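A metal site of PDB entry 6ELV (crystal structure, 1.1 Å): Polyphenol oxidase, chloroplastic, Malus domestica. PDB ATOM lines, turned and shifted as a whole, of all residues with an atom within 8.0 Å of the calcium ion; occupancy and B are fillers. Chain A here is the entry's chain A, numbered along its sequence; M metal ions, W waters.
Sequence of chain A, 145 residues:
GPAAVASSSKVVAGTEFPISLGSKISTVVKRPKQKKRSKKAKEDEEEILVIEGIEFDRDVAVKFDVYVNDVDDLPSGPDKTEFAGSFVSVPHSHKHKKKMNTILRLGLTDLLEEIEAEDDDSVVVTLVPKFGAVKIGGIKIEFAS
The calcium ion is bound by the side-chain carboxylate (OD2) of Asp 72 (2.4 Å).
The calcium ion is bound by water W1 (2.4 Å).
The calcium ion is bound by the side-chain carboxylate (OD2) of Asp 120 (2.4 Å).
The calcium ion is bound by water W2, 2.5 Å away.
The calcium ion is bound by the side-chain carboxylate (OD2) of Asp 70 (2.5 Å).
The calcium ion is bound by OD1 of Asp 70 (2.5 Å).
OD1 of Asp 120 is bound to the calcium ion, 2.6 Å away.
Water W1 lies within hydrogen-bond range of O of Glu 116 (2.8 Å) and OD1 of Asp 119 (2.8 Å).
Three residues have an atom within 4 Å of the calcium ion: Asp 70, Asp 72 and Asp 120.
Along chain A the residues within 4 Å of the calcium ion span positions 70 to 120.
The nearest printed residue that does not touch the calcium ion is Asp 119 (4.4 Å).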
ATOM      1  N   ASN A  69      18.088  -9.481 -14.667  1.00  0.00           N
ATOM      2  CA  ASN A  69      17.741  -8.727 -13.464  1.00  0.00           C
ATOM      3  C   ASN A  69      16.744  -9.507 -12.627  1.00  0.00           C
ATOM      4  O   ASN A  69      16.088 -10.436 -13.102  1.00  0.00           O
ATOM      5  CB  ASN A  69      17.246  -7.285 -13.746  1.00  0.00           C
ATOM      6  CG  ASN A  69      15.876  -7.216 -14.417  1.00  0.00           C
ATOM      7  OD1 ASN A  69      15.784  -7.133 -15.651  1.00  0.00           O
ATOM      8  ND2 ASN A  69      14.810  -7.179 -13.633  1.00  0.00           N
ATOM      9  N   ASP A  70      16.639  -9.078 -11.370  1.00  0.00           N
ATOM     10  CA  ASP A  70      15.715  -9.670 -10.405  1.00  0.00           C
ATOM     11  C   ASP A  70      14.285  -9.409 -10.860  1.00  0.00           C
ATOM     12  O   ASP A  70      13.902  -8.276 -11.163  1.00  0.00           O
ATOM     13  CB  ASP A  70      16.006  -9.012  -9.051  1.00  0.00           C
ATOM     14  CG  ASP A  70      15.248  -9.634  -7.901  1.00  0.00           C
ATOM     15  OD1 ASP A  70      14.006  -9.727  -7.973  1.00  0.00           O
ATOM     16  OD2 ASP A  70      15.896  -9.979  -6.882  1.00  0.00           O
ATOM     17  N   VAL A  71      13.488 -10.486 -10.897  1.00  0.00           N
ATOM     18  CA  VAL A  71      12.114 -10.432 -11.372  1.00  0.00           C
ATOM     19  C   VAL A  71      11.243  -9.475 -10.580  1.00  0.00           C
ATOM     20  O   VAL A  71      10.219  -9.001 -11.081  1.00  0.00           O
ATOM     21  CB  VAL A  71      11.528 -11.863 -11.383  1.00  0.00           C
ATOM     22  CG1 VAL A  71      11.338 -12.388  -9.958  1.00  0.00           C
ATOM     23  CG2 VAL A  71      10.244 -11.926 -12.190  1.00  0.00           C
ATOM     24  N   ASP A  72      11.616  -9.165  -9.349  1.00  0.00           N
ATOM     25  CA  ASP A  72      10.824  -8.285  -8.508  1.00  0.00           C
ATOM     26  C   ASP A  72      11.174  -6.805  -8.670  1.00  0.00           C
ATOM     27  O   ASP A  72      10.539  -5.949  -8.049  1.00  0.00           O
ATOM     28  CB  ASP A  72      11.030  -8.691  -7.054  1.00  0.00           C
ATOM     29  CG  ASP A  72      10.707 -10.160  -6.827  1.00  0.00           C
ATOM     30  OD1 ASP A  72       9.552 -10.553  -7.132  1.00  0.00           O
ATOM     31  OD2 ASP A  72      11.583 -10.916  -6.352  1.00  0.00           O
ATOM     32  N   ASP A  73      12.189  -6.477  -9.477  1.00  0.00           N
ATOM     33  CA  ASP A  73      12.501  -5.079  -9.718  1.00  0.00           C
ATOM     34  C   ASP A  73      11.360  -4.408 -10.472  1.00  0.00           C
ATOM     35  O   ASP A  73      10.719  -5.020 -11.324  1.00  0.00           O
ATOM     36  CB  ASP A  73      13.719  -4.957 -10.640  1.00  0.00           C
ATOM     37  CG  ASP A  73      14.998  -5.463 -10.034  1.00  0.00           C
ATOM     38  OD1 ASP A  73      15.072  -5.770  -8.827  1.00  0.00           O
ATOM     39  OD2 ASP A  73      15.974  -5.529 -10.832  1.00  0.00           O
ATOM     40  N   ILE A 115      23.456 -10.268  -8.114  1.00  0.00           N
ATOM     41  CA  ILE A 115      22.240  -9.463  -8.141  1.00  0.00           C
ATOM     42  C   ILE A 115      21.314  -9.768  -6.973  1.00  0.00           C
ATOM     43  O   ILE A 115      20.300  -9.087  -6.814  1.00  0.00           O
ATOM     44  CB  ILE A 115      21.492  -9.536  -9.488  1.00  0.00           C
ATOM     45  CG1 ILE A 115      20.867 -10.909  -9.722  1.00  0.00           C
ATOM     46  CG2 ILE A 115      22.428  -9.157 -10.617  1.00  0.00           C
ATOM     47  CD1 ILE A 115      19.904 -10.936 -10.890  1.00  0.00           C
ATOM     48  N   GLU A 116      21.651 -10.772  -6.170  1.00  0.00           N
ATOM     49  CA  GLU A 116      20.892 -11.152  -4.975  1.00  0.00           C
ATOM     50  C   GLU A 116      19.484 -11.663  -5.315  1.00  0.00           C
ATOM     51  O   GLU A 116      18.496 -11.293  -4.679  1.00  0.00           O
ATOM     52  CB  GLU A 116      20.878 -10.035  -3.932  1.00  0.00           C
ATOM     53  CG  GLU A 116      22.276  -9.614  -3.527  1.00  0.00           C
ATOM     54  CD  GLU A 116      22.281  -8.633  -2.381  1.00  0.00           C
ATOM     55  OE1 GLU A 116      21.699  -7.542  -2.525  1.00  0.00           O
ATOM     56  OE2 GLU A 116      22.874  -8.959  -1.325  1.00  0.00           O
ATOM     57  N   ALA A 117      19.420 -12.528  -6.329  1.00  0.00           N
ATOM     58  CA  ALA A 117      18.199 -13.165  -6.779  1.00  0.00           C
ATOM     59  C   ALA A 117      18.176 -14.670  -6.512  1.00  0.00           C
ATOM     60  O   ALA A 117      17.341 -15.388  -7.069  1.00  0.00           O
ATOM     61  CB  ALA A 117      17.975 -12.885  -8.266  1.00  0.00           C
ATOM     62  N   GLU A 118      19.096 -15.169  -5.663  1.00  0.00           N
ATOM     63  CA  GLU A 118      19.244 -16.613  -5.491  1.00  0.00           C
ATOM     64  C   GLU A 118      17.998 -17.258  -4.897  1.00  0.00           C
ATOM     65  O   GLU A 118      17.816 -18.470  -5.041  1.00  0.00           O
ATOM     66  CB  GLU A 118      20.409 -16.934  -4.567  1.00  0.00           C
ATOM     67  CG  GLU A 118      21.785 -16.704  -5.155  1.00  0.00           C
ATOM     68  CD  GLU A 118      22.886 -16.942  -4.128  1.00  0.00           C
ATOM     69  OE1 GLU A 118      23.044 -16.068  -3.245  1.00  0.00           O
ATOM     70  OE2 GLU A 118      23.579 -17.973  -4.200  1.00  0.00           O
ATOM     71  N   ASP A 119      17.171 -16.470  -4.209  1.00  0.00           N
ATOM     72  CA  ASP A 119      15.958 -16.922  -3.546  1.00  0.00           C
ATOM     73  C   ASP A 119      14.743 -16.886  -4.452  1.00  0.00           C
ATOM     74  O   ASP A 119      13.647 -17.245  -4.010  1.00  0.00           O
ATOM     75  CB  ASP A 119      15.675 -15.993  -2.371  1.00  0.00           C
ATOM     76  CG  ASP A 119      15.460 -14.539  -2.805  1.00  0.00           C
ATOM     77  OD1 ASP A 119      16.412 -13.927  -3.327  1.00  0.00           O
ATOM     78  OD2 ASP A 119      14.335 -14.023  -2.642  1.00  0.00           O
ATOM     79  N   ASP A 120      14.876 -16.403  -5.691  1.00  0.00           N
ATOM     80  CA  ASP A 120      13.740 -16.211  -6.576  1.00  0.00           C
ATOM     81  C   ASP A 120      13.534 -17.460  -7.454  1.00  0.00           C
ATOM     82  O   ASP A 120      14.460 -18.229  -7.714  1.00  0.00           O
ATOM     83  CB  ASP A 120      13.961 -15.002  -7.490  1.00  0.00           C
ATOM     84  CG  ASP A 120      14.001 -13.663  -6.744  1.00  0.00           C
ATOM     85  OD1 ASP A 120      13.488 -13.558  -5.612  1.00  0.00           O
ATOM     86  OD2 ASP A 120      14.533 -12.710  -7.323  1.00  0.00           O
ATOM     87  N   ASP A 121      12.298 -17.628  -7.936  1.00  0.00           N
ATOM     88  CA  ASP A 121      11.965 -18.759  -8.791  1.00  0.00           C
ATOM     89  C   ASP A 121      12.097 -18.451 -10.279  1.00  0.00           C
ATOM     90  O   ASP A 121      12.021 -19.381 -11.091  1.00  0.00           O
ATOM     91  CB  ASP A 121      10.530 -19.229  -8.514  1.00  0.00           C
ATOM     92  CG  ASP A 121      10.414 -20.021  -7.227  1.00  0.00           C
ATOM     93  OD1 ASP A 121      11.337 -20.794  -6.914  1.00  0.00           O
ATOM     94  OD2 ASP A 121       9.398 -19.867  -6.525  1.00  0.00           O
ATOM     95  N   SER A 122      12.273 -17.190 -10.640  1.00  0.00           N
ATOM     96  CA  SER A 122      12.414 -16.788 -12.033  1.00  0.00           C
ATOM     97  C   SER A 122      13.281 -15.546 -12.051  1.00  0.00           C
ATOM     98  O   SER A 122      13.527 -14.940 -11.001  1.00  0.00           O
ATOM     99  CB  SER A 122      11.058 -16.466 -12.652  1.00  0.00           C
ATOM    100  OG  SER A 122      10.416 -15.433 -11.941  1.00  0.00           O
HETATM  101 CA    CA M   1      13.913 -10.957  -5.767  1.00  0.00          CA
HETATM  102  O   HOH W   1      15.770 -11.418  -4.301  1.00  0.00           O
HETATM  103  O   HOH W   2      12.950 -11.243  -3.510  1.00  0.00           O
